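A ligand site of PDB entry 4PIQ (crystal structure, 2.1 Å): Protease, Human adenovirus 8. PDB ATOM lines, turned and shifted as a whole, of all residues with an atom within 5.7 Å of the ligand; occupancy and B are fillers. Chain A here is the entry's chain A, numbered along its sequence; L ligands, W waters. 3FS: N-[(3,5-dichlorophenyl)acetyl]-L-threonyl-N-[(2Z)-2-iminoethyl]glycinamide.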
ATOM      1  N   SER A   1     -21.283  -8.368 -29.578  1.00  0.00           N
ATOM      2  CA  SER A   1     -22.744  -8.339 -29.544  1.00  0.00           C
ATOM      3  C   SER A   1     -23.252  -8.455 -28.090  1.00  0.00           C
ATOM      4  O   SER A   1     -23.240  -9.547 -27.516  1.00  0.00           O
ATOM      5  CB  SER A   1     -23.314  -9.458 -30.420  1.00  0.00           C
ATOM      6  OG  SER A   1     -24.708  -9.335 -30.663  1.00  0.00           O
ATOM      7  N   GLY A   2     -23.685  -7.336 -27.512  1.00  0.00           N
ATOM      8  CA  GLY A   2     -24.222  -7.301 -26.155  1.00  0.00           C
ATOM      9  C   GLY A   2     -23.182  -7.227 -25.049  1.00  0.00           C
ATOM     10  O   GLY A   2     -22.080  -6.706 -25.258  1.00  0.00           O
ATOM     11  N   SER A   3     -23.556  -7.730 -23.838  1.00  0.00           N
ATOM     12  CA  SER A   3     -22.714  -7.722 -22.630  1.00  0.00           C
ATOM     13  C   SER A   3     -22.187  -9.105 -22.246  1.00  0.00           C
ATOM     14  O   SER A   3     -22.946 -10.068 -22.238  1.00  0.00           O
ATOM     15  CB  SER A   3     -23.487  -7.138 -21.448  1.00  0.00           C
ATOM     16  OG  SER A   3     -23.654  -5.728 -21.513  1.00  0.00           O
ATOM     17  N   SER A   4     -20.885  -9.192 -21.905  1.00  0.00           N
ATOM     18  CA  SER A   4     -20.222 -10.448 -21.480  1.00  0.00           C
ATOM     19  C   SER A   4     -20.452 -10.607 -19.964  1.00  0.00           C
ATOM     20  O   SER A   4     -20.760  -9.627 -19.282  1.00  0.00           O
ATOM     21  CB  SER A   4     -18.720 -10.389 -21.770  1.00  0.00           C
ATOM     22  OG  SER A   4     -18.073  -9.421 -20.953  1.00  0.00           O
ATOM     23  N   GLU A   5     -20.249 -11.799 -19.420  1.00  0.00           N
ATOM     24  CA  GLU A   5     -20.441 -12.013 -17.983  1.00  0.00           C
ATOM     25  C   GLU A   5     -19.460 -11.216 -17.106  1.00  0.00           C
ATOM     26  O   GLU A   5     -19.864 -10.740 -16.031  1.00  0.00           O
ATOM     27  CB  GLU A   5     -20.448 -13.501 -17.618  1.00  0.00           C
ATOM     28  CG  GLU A   5     -19.262 -14.310 -18.105  1.00  0.00           C
ATOM     29  CD  GLU A   5     -19.076 -15.608 -17.349  1.00  0.00           C
ATOM     30  OE1 GLU A   5     -18.855 -16.657 -17.997  1.00  0.00           O
ATOM     31  OE2 GLU A   5     -19.179 -15.580 -16.097  1.00  0.00           O
ATOM     32  N   GLN A   6     -18.217 -10.997 -17.581  1.00  0.00           N
ATOM     33  CA  GLN A   6     -17.163 -10.228 -16.884  1.00  0.00           C
ATOM     34  C   GLN A   6     -17.576  -8.775 -16.703  1.00  0.00           C
ATOM     35  O   GLN A   6     -17.419  -8.205 -15.604  1.00  0.00           O
ATOM     36  CB  GLN A   6     -15.814 -10.270 -17.651  1.00  0.00           C
ATOM     37  CG  GLN A   6     -15.193 -11.665 -17.810  1.00  0.00           C
ATOM     38  CD  GLN A   6     -15.875 -12.563 -18.831  1.00  0.00           C
ATOM     39  OE1 GLN A   6     -16.453 -12.104 -19.818  1.00  0.00           O
ATOM     40  NE2 GLN A   6     -15.824 -13.865 -18.599  1.00  0.00           N
ATOM     41  N   THR A  24     -22.938 -14.679 -12.138  1.00  0.00           N
ATOM     42  CA  THR A  24     -23.576 -14.774 -13.460  1.00  0.00           C
ATOM     43  C   THR A  24     -23.647 -16.216 -13.859  1.00  0.00           C
ATOM     44  O   THR A  24     -22.713 -16.979 -13.639  1.00  0.00           O
ATOM     45  CB  THR A  24     -22.892 -13.886 -14.500  1.00  0.00           C
ATOM     46  OG1 THR A  24     -21.517 -14.289 -14.615  1.00  0.00           O
ATOM     47  CG2 THR A  24     -22.955 -12.401 -14.160  1.00  0.00           C
ATOM     48  N   HIS A  25     -24.814 -16.615 -14.404  1.00  0.00           N
ATOM     49  CA  HIS A  25     -25.072 -17.993 -14.767  1.00  0.00           C
ATOM     50  C   HIS A  25     -25.851 -18.122 -16.049  1.00  0.00           C
ATOM     51  O   HIS A  25     -26.483 -17.184 -16.515  1.00  0.00           O
ATOM     52  CB  HIS A  25     -25.885 -18.659 -13.648  1.00  0.00           C
ATOM     53  CG  HIS A  25     -25.225 -18.667 -12.300  1.00  0.00           C
ATOM     54  ND1 HIS A  25     -25.383 -17.610 -11.414  1.00  0.00           N
ATOM     55  CD2 HIS A  25     -24.505 -19.639 -11.700  1.00  0.00           C
ATOM     56  CE1 HIS A  25     -24.723 -17.957 -10.330  1.00  0.00           C
ATOM     57  NE2 HIS A  25     -24.168 -19.163 -10.454  1.00  0.00           N
ATOM     58  N   ASP A  26     -25.867 -19.346 -16.555  1.00  0.00           N
ATOM     59  CA  ASP A  26     -26.658 -19.771 -17.678  1.00  0.00           C
ATOM     60  C   ASP A  26     -28.020 -20.261 -17.077  1.00  0.00           C
ATOM     61  O   ASP A  26     -28.213 -20.162 -15.857  1.00  0.00           O
ATOM     62  CB  ASP A  26     -25.909 -20.873 -18.462  1.00  0.00           C
ATOM     63  CG  ASP A  26     -25.740 -22.261 -17.823  1.00  0.00           C
ATOM     64  OD1 ASP A  26     -26.088 -22.414 -16.632  1.00  0.00           O
ATOM     65  OD2 ASP A  26     -25.283 -23.181 -18.526  1.00  0.00           O
ATOM     66  N   LYS A  27     -28.925 -20.800 -17.921  1.00  0.00           N
ATOM     67  CA  LYS A  27     -30.262 -21.289 -17.548  1.00  0.00           C
ATOM     68  C   LYS A  27     -30.296 -22.313 -16.392  1.00  0.00           C
ATOM     69  O   LYS A  27     -31.344 -22.442 -15.765  1.00  0.00           O
ATOM     70  CB  LYS A  27     -31.047 -21.829 -18.775  1.00  0.00           C
ATOM     71  CG  LYS A  27     -30.488 -23.061 -19.466  1.00  0.00           C
ATOM     72  CD  LYS A  27     -31.531 -23.629 -20.425  1.00  0.00           C
ATOM     73  CE  LYS A  27     -31.047 -24.813 -21.227  1.00  0.00           C
ATOM     74  NZ  LYS A  27     -31.949 -25.104 -22.378  1.00  0.00           N
ATOM     75  N   ASN A  44     -28.746 -16.219 -17.719  1.00  0.00           N
ATOM     76  CA  ASN A  44     -28.978 -16.278 -19.148  1.00  0.00           C
ATOM     77  C   ASN A  44     -30.080 -17.286 -19.463  1.00  0.00           C
ATOM     78  O   ASN A  44     -30.139 -18.334 -18.822  1.00  0.00           O
ATOM     79  CB  ASN A  44     -27.690 -16.691 -19.888  1.00  0.00           C
ATOM     80  CG  ASN A  44     -27.672 -16.224 -21.316  1.00  0.00           C
ATOM     81  OD1 ASN A  44     -28.119 -16.922 -22.250  1.00  0.00           O
ATOM     82  ND2 ASN A  44     -27.121 -15.032 -21.515  1.00  0.00           N
ATOM     83  N   ALA A  46     -30.286 -19.122 -22.105  1.00  0.00           N
ATOM     84  CA  ALA A  46     -29.684 -20.282 -22.724  1.00  0.00           C
ATOM     85  C   ALA A  46     -28.577 -20.889 -21.868  1.00  0.00           C
ATOM     86  O   ALA A  46     -28.142 -20.282 -20.898  1.00  0.00           O
ATOM     87  CB  ALA A  46     -29.167 -19.911 -24.114  1.00  0.00           C
ATOM     88  N   GLY A  47     -28.180 -22.103 -22.220  1.00  0.00           N
ATOM     89  CA  GLY A  47     -27.077 -22.806 -21.549  1.00  0.00           C
ATOM     90  C   GLY A  47     -25.768 -22.320 -22.114  1.00  0.00           C
ATOM     91  O   GLY A  47     -25.699 -21.958 -23.291  1.00  0.00           O
ATOM     92  N   ARG A  48     -24.702 -22.323 -21.284  1.00  0.00           N
ATOM     93  CA  ARG A  48     -23.342 -21.870 -21.625  1.00  0.00           C
ATOM     94  C   ARG A  48     -22.845 -22.318 -22.996  1.00  0.00           C
ATOM     95  O   ARG A  48     -22.148 -21.543 -23.673  1.00  0.00           O
ATOM     96  CB  ARG A  48     -22.331 -22.280 -20.547  1.00  0.00           C
ATOM     97  CG  ARG A  48     -22.206 -21.278 -19.426  1.00  0.00           C
ATOM     98  CD  ARG A  48     -21.099 -21.698 -18.471  1.00  0.00           C
ATOM     99  NE  ARG A  48     -21.167 -20.985 -17.198  1.00  0.00           N
ATOM    100  CZ  ARG A  48     -20.593 -19.812 -16.972  1.00  0.00           C
ATOM    101  NH1 ARG A  48     -20.715 -19.221 -15.789  1.00  0.00           N
ATOM    102  NH2 ARG A  48     -19.898 -19.198 -17.927  1.00  0.00           N
ATOM    103  N   GLU A  49     -23.200 -23.570 -23.387  1.00  0.00           N
ATOM    104  CA  GLU A  49     -22.853 -24.243 -24.645  1.00  0.00           C
ATOM    105  C   GLU A  49     -23.340 -23.494 -25.928  1.00  0.00           C
ATOM    106  O   GLU A  49     -22.672 -23.577 -26.962  1.00  0.00           O
ATOM    107  CB  GLU A  49     -23.337 -25.719 -24.644  1.00  0.00           C
ATOM    108  CG  GLU A  49     -24.834 -25.962 -24.778  1.00  0.00           C
ATOM    109  CD  GLU A  49     -25.704 -25.728 -23.554  1.00  0.00           C
ATOM    110  OE1 GLU A  49     -26.895 -25.405 -23.743  1.00  0.00           O
ATOM    111  OE2 GLU A  49     -25.219 -25.905 -22.415  1.00  0.00           O
ATOM    112  N   THR A  50     -24.470 -22.777 -25.847  1.00  0.00           N
ATOM    113  CA  THR A  50     -24.988 -21.989 -26.977  1.00  0.00           C
ATOM    114  C   THR A  50     -24.117 -20.718 -27.199  1.00  0.00           C
ATOM    115  O   THR A  50     -24.059 -20.198 -28.309  1.00  0.00           O
ATOM    116  CB  THR A  50     -26.417 -21.541 -26.706  1.00  0.00           C
ATOM    117  OG1 THR A  50     -26.414 -20.665 -25.585  1.00  0.00           O
ATOM    118  CG2 THR A  50     -27.384 -22.707 -26.498  1.00  0.00           C
ATOM    119  N   GLY A  51     -23.530 -20.217 -26.111  1.00  0.00           N
ATOM    120  CA  GLY A  51     -22.730 -18.997 -26.093  1.00  0.00           C
ATOM    121  C   GLY A  51     -23.463 -17.865 -25.399  1.00  0.00           C
ATOM    122  O   GLY A  51     -22.866 -16.823 -25.137  1.00  0.00           O
ATOM    123  N   GLY A  52     -24.736 -18.090 -25.092  1.00  0.00           N
ATOM    124  CA  GLY A  52     -25.605 -17.118 -24.443  1.00  0.00           C
ATOM    125  C   GLY A  52     -26.522 -16.404 -25.415  1.00  0.00           C
ATOM    126  O   GLY A  52     -26.146 -16.173 -26.571  1.00  0.00           O
ATOM    127  N   VAL A  53     -27.735 -16.055 -24.957  1.00  0.00           N
ATOM    128  CA  VAL A  53     -28.752 -15.391 -25.783  1.00  0.00           C
ATOM    129  C   VAL A  53     -29.336 -14.144 -25.085  1.00  0.00           C
ATOM    130  O   VAL A  53     -29.116 -13.028 -25.568  1.00  0.00           O
ATOM    131  CB  VAL A  53     -29.852 -16.406 -26.235  1.00  0.00           C
ATOM    132  CG1 VAL A  53     -31.057 -15.709 -26.883  1.00  0.00           C
ATOM    133  CG2 VAL A  53     -29.295 -17.455 -27.178  1.00  0.00           C
ATOM    134  N   HIS A  54     -30.086 -14.319 -23.962  1.00  0.00           N
ATOM    135  CA  HIS A  54     -30.723 -13.168 -23.294  1.00  0.00           C
ATOM    136  C   HIS A  54     -30.395 -13.071 -21.798  1.00  0.00           C
ATOM    137  O   HIS A  54     -30.362 -14.091 -21.117  1.00  0.00           O
ATOM    138  CB  HIS A  54     -32.246 -13.247 -23.569  1.00  0.00           C
ATOM    139  CG  HIS A  54     -33.090 -12.166 -22.965  1.00  0.00           C
ATOM    140  ND1 HIS A  54     -32.766 -10.831 -23.097  1.00  0.00           N
ATOM    141  CD2 HIS A  54     -34.284 -12.267 -22.351  1.00  0.00           C
ATOM    142  CE1 HIS A  54     -33.724 -10.170 -22.476  1.00  0.00           C
ATOM    143  NE2 HIS A  54     -34.669 -10.996 -22.038  1.00  0.00           N
ATOM    144  N   TRP A  55     -30.179 -11.867 -21.277  1.00  0.00           N
ATOM    145  CA  TRP A  55     -29.878 -11.700 -19.856  1.00  0.00           C
ATOM    146  C   TRP A  55     -31.130 -11.382 -18.973  1.00  0.00           C
ATOM    147  O   TRP A  55     -31.910 -10.507 -19.349  1.00  0.00           O
ATOM    148  CB  TRP A  55     -28.803 -10.615 -19.649  1.00  0.00           C
ATOM    149  CG  TRP A  55     -27.421 -11.031 -20.098  1.00  0.00           C
ATOM    150  CD1 TRP A  55     -26.711 -10.507 -21.138  1.00  0.00           C
ATOM    151  CD2 TRP A  55     -26.592 -12.038 -19.507  1.00  0.00           C
ATOM    152  NE1 TRP A  55     -25.493 -11.141 -21.236  1.00  0.00           N
ATOM    153  CE2 TRP A  55     -25.400 -12.099 -20.267  1.00  0.00           C
ATOM    154  CE3 TRP A  55     -26.755 -12.926 -18.430  1.00  0.00           C
ATOM    155  CZ2 TRP A  55     -24.354 -12.959 -19.941  1.00  0.00           C
ATOM    156  CZ3 TRP A  55     -25.711 -13.790 -18.117  1.00  0.00           C
ATOM    157  CH2 TRP A  55     -24.541 -13.821 -18.877  1.00  0.00           C
ATOM    158  N   PHE A  73     -37.679  -6.774 -21.062  1.00  0.00           N
ATOM    159  CA  PHE A  73     -38.790  -6.818 -22.012  1.00  0.00           C
ATOM    160  C   PHE A  73     -40.173  -7.060 -21.346  1.00  0.00           C
ATOM    161  O   PHE A  73     -41.205  -6.876 -22.013  1.00  0.00           O
ATOM    162  CB  PHE A  73     -38.515  -7.909 -23.053  1.00  0.00           C
ATOM    163  CG  PHE A  73     -37.438  -7.603 -24.082  1.00  0.00           C
ATOM    164  CD1 PHE A  73     -36.573  -8.586 -24.519  1.00  0.00           C
ATOM    165  CD2 PHE A  73     -37.316  -6.322 -24.623  1.00  0.00           C
ATOM    166  CE1 PHE A  73     -35.616  -8.323 -25.485  1.00  0.00           C
ATOM    167  CE2 PHE A  73     -36.366  -6.052 -25.606  1.00  0.00           C
ATOM    168  CZ  PHE A  73     -35.511  -7.049 -26.020  1.00  0.00           C
ATOM    169  N   GLN A 115     -36.971  -1.873 -22.578  1.00  0.00           N
ATOM    170  CA  GLN A 115     -36.028  -2.037 -23.673  1.00  0.00           C
ATOM    171  C   GLN A 115     -36.701  -2.051 -25.049  1.00  0.00           C
ATOM    172  O   GLN A 115     -37.813  -2.581 -25.188  1.00  0.00           O
ATOM    173  CB  GLN A 115     -35.222  -3.306 -23.432  1.00  0.00           C
ATOM    174  CG  GLN A 115     -33.921  -3.363 -24.230  1.00  0.00           C
ATOM    175  CD  GLN A 115     -33.239  -4.683 -24.084  1.00  0.00           C
ATOM    176  OE1 GLN A 115     -32.572  -5.178 -25.018  1.00  0.00           O
ATOM    177  NE2 GLN A 115     -33.367  -5.275 -22.924  1.00  0.00           N
ATOM    178  N   SER A 119     -32.656  -3.514 -29.344  1.00  0.00           N
ATOM    179  CA  SER A 119     -31.600  -3.234 -28.379  1.00  0.00           C
ATOM    180  C   SER A 119     -30.874  -4.479 -27.848  1.00  0.00           C
ATOM    181  O   SER A 119     -31.451  -5.570 -27.758  1.00  0.00           O
ATOM    182  CB  SER A 119     -32.127  -2.378 -27.240  1.00  0.00           C
ATOM    183  OG  SER A 119     -31.112  -2.101 -26.304  1.00  0.00           O
ATOM    184  N   ALA A 120     -29.581  -4.284 -27.542  1.00  0.00           N
ATOM    185  CA  ALA A 120     -28.684  -5.317 -27.007  1.00  0.00           C
ATOM    186  C   ALA A 120     -28.215  -4.987 -25.579  1.00  0.00           C
ATOM    187  O   ALA A 120     -27.281  -5.623 -25.085  1.00  0.00           O
ATOM    188  CB  ALA A 120     -27.491  -5.539 -27.937  1.00  0.00           C
ATOM    189  N   ALA A 121     -28.899  -3.993 -24.913  1.00  0.00           N
ATOM    190  CA  ALA A 121     -28.653  -3.554 -23.545  1.00  0.00           C
ATOM    191  C   ALA A 121     -29.373  -4.377 -22.445  1.00  0.00           C
ATOM    192  O   ALA A 121     -29.496  -3.857 -21.342  1.00  0.00           O
ATOM    193  CB  ALA A 121     -29.001  -2.068 -23.403  1.00  0.00           C
ATOM    194  N   CYS A 122     -29.814  -5.645 -22.707  1.00  0.00           N
ATOM    195  CA  CYS A 122     -30.509  -6.434 -21.664  1.00  0.00           C
ATOM    196  C   CYS A 122     -29.663  -6.662 -20.423  1.00  0.00           C
ATOM    197  O   CYS A 122     -30.160  -6.436 -19.322  1.00  0.00           O
ATOM    198  CB  CYS A 122     -31.081  -7.745 -22.206  1.00  0.00           C
ATOM    199  SG  CYS A 122     -29.958  -8.693 -23.243  1.00  0.00           S
ATOM    200  N   GLY A 123     -28.391  -7.048 -20.601  1.00  0.00           N
ATOM    201  CA  GLY A 123     -27.447  -7.209 -19.497  1.00  0.00           C
ATOM    202  C   GLY A 123     -27.348  -5.957 -18.633  1.00  0.00           C
ATOM    203  O   GLY A 123     -27.421  -6.045 -17.413  1.00  0.00           O
HETATM  204  C12 3FS L   1     -21.308 -14.701 -22.319  1.00  0.00           C
HETATM  205  C13 3FS L   1     -20.906 -16.156 -22.160  1.00  0.00           C
HETATM  206  C15 3FS L   1     -21.908 -16.797 -21.190  1.00  0.00           C
HETATM  207  C16 3FS L   1     -23.019 -17.521 -21.671  1.00  0.00           C
HETATM  208  C17 3FS L   1     -23.984 -18.056 -20.778  1.00  0.00           C
HETATM  209  C18 3FS L   1     -23.851 -17.824 -19.401  1.00  0.00           C
HETATM  210  C19 3FS L   1     -22.766 -17.086 -18.913  1.00  0.00           C
HETATM  211  C20 3FS L   1     -21.794 -16.572 -19.808  1.00  0.00           C
HETATM  212  O14 3FS L   1     -20.860 -13.893 -21.504  1.00  0.00           O
HETATM  213 CL1  3FS L   1     -22.600 -16.799 -17.204  1.00  0.00          CL
HETATM  214 CL2  3FS L   1     -25.352 -18.966 -21.400  1.00  0.00          CL
HETATM  215  N9  3FS L   1     -22.179 -14.408 -23.327  1.00  0.00           N
HETATM  216  C8  3FS L   1     -22.738 -13.069 -23.619  1.00  0.00           C
HETATM  217  C6  3FS L   1     -24.268 -13.095 -23.758  1.00  0.00           C
HETATM  218  O7  3FS L   1     -24.887 -14.120 -23.485  1.00  0.00           O
HETATM  219  C10 3FS L   1     -22.127 -12.440 -24.924  1.00  0.00           C
HETATM  220  O26 3FS L   1     -22.591 -13.170 -26.080  1.00  0.00           O
HETATM  221  C11 3FS L   1     -20.583 -12.274 -24.932  1.00  0.00           C
HETATM  222  N5  3FS L   1     -24.887 -11.956 -24.210  1.00  0.00           N
HETATM  223  C4  3FS L   1     -26.328 -11.807 -24.431  1.00  0.00           C
HETATM  224  C2  3FS L   1     -26.700 -10.366 -24.683  1.00  0.00           C
HETATM  225  O3  3FS L   1     -26.050  -9.487 -24.125  1.00  0.00           O
HETATM  226  C24 3FS L   1     -29.224  -8.288 -24.818  1.00  0.00           C
HETATM  227  N25 3FS L   1     -30.253  -7.804 -25.252  1.00  0.00           N
HETATM  228  C23 3FS L   1     -28.260  -8.785 -25.824  1.00  0.00           C
HETATM  229  N1  3FS L   1     -27.752 -10.118 -25.516  1.00  0.00           N
HETATM  230  O   HOH W   1     -24.967 -11.658 -27.628  1.00  0.00           O
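C24 of the ligand is covalently linked to SG of Cys 122.
An oxygen (O14) of the ligand sits at hydrogen-bond distance from the backbone NH (N) of Glu 5, at 3.0 Å.
N of Ser 3 is in hydrogen-bond range of O3 of the ligand (3.1 Å).
The backbone carbonyl oxygen of Ser 3 sits close to a nitrogen (N5) of the ligand.
The backbone carbonyl oxygen of Gly 51 lies within hydrogen-bond range of a nitrogen (N9) of the ligand (3.1 Å).
The side-chain amide nitrogen (ND2) of Asn 44 lies within hydrogen-bond range of an oxygen (O7) of the ligand (3.1 Å).
NE1 of Trp 55 sits close to O3 of the ligand (3.4 Å).
A nitrogen (N1) of the ligand lies within hydrogen-bond range of the backbone carbonyl oxygen of Val 53 (3.2 Å).
OE1 of Glu 5 is in salt-bridge range of NH2 of Arg 48 (2.7 Å).
The indole nitrogen (NE1) of Trp 55 is in hydrogen-bond range of the backbone carbonyl oxygen (O) of Ser 3, at 2.9 Å.
OD1 of Asn 44 is in hydrogen-bond range of N of Ala 46 (3.1 Å).
N of Val 53 lies within hydrogen-bond range of OD1 of Asn 44.
The backbone carbonyl oxygen of His 25 lies within hydrogen-bond range of the backbone NH of Asn 44, 2.7 Å away.
The backbone carbonyl oxygen (O) of Asn 44 is in hydrogen-bond range of the backbone NH (N) of Lys 27, at 2.9 Å.
O of Ala 46 is in hydrogen-bond range of N of Lys 27 (3.1 Å).
The side-chain amide oxygen of Gln 115 lies close to the backbone carbonyl oxygen of Ser 119 (3.0 Å).
Merely in contact with the ligand: Ala 46 (3.1 Å), Gly 52 (3.2 Å), Ala 120 (3.3 Å), Arg 48 (3.4 Å), Gly 47 (3.5 Å), Gly 2 (3.5 Å), Ser 4 (3.5 Å), Gln 115 (3.5 Å), Asp 26 (3.5 Å), Thr 24 (3.6 Å), Ser 119 (3.6 Å), His 25 (3.6 Å) and Ser 1 (3.95 Å).
20 residues have an atom within 4 Å of the ligand: Ser 1, Gly 2, Ser 3, Ser 4, Glu 5, Thr 24, His 25, Asp 26, Asn 44, Ala 46, Gly 47, Arg 48, Gly 51, Gly 52, Val 53, Trp 55, Gln 115, Ser 119, Ala 120 and Cys 122.
The nearest printed residue that does not touch the ligand is Ala 121 (4.1 Å).
Water W1 lies within hydrogen-bond range of O of Ser 1 (2.7 Å) and O26 of the ligand (3.2 Å).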
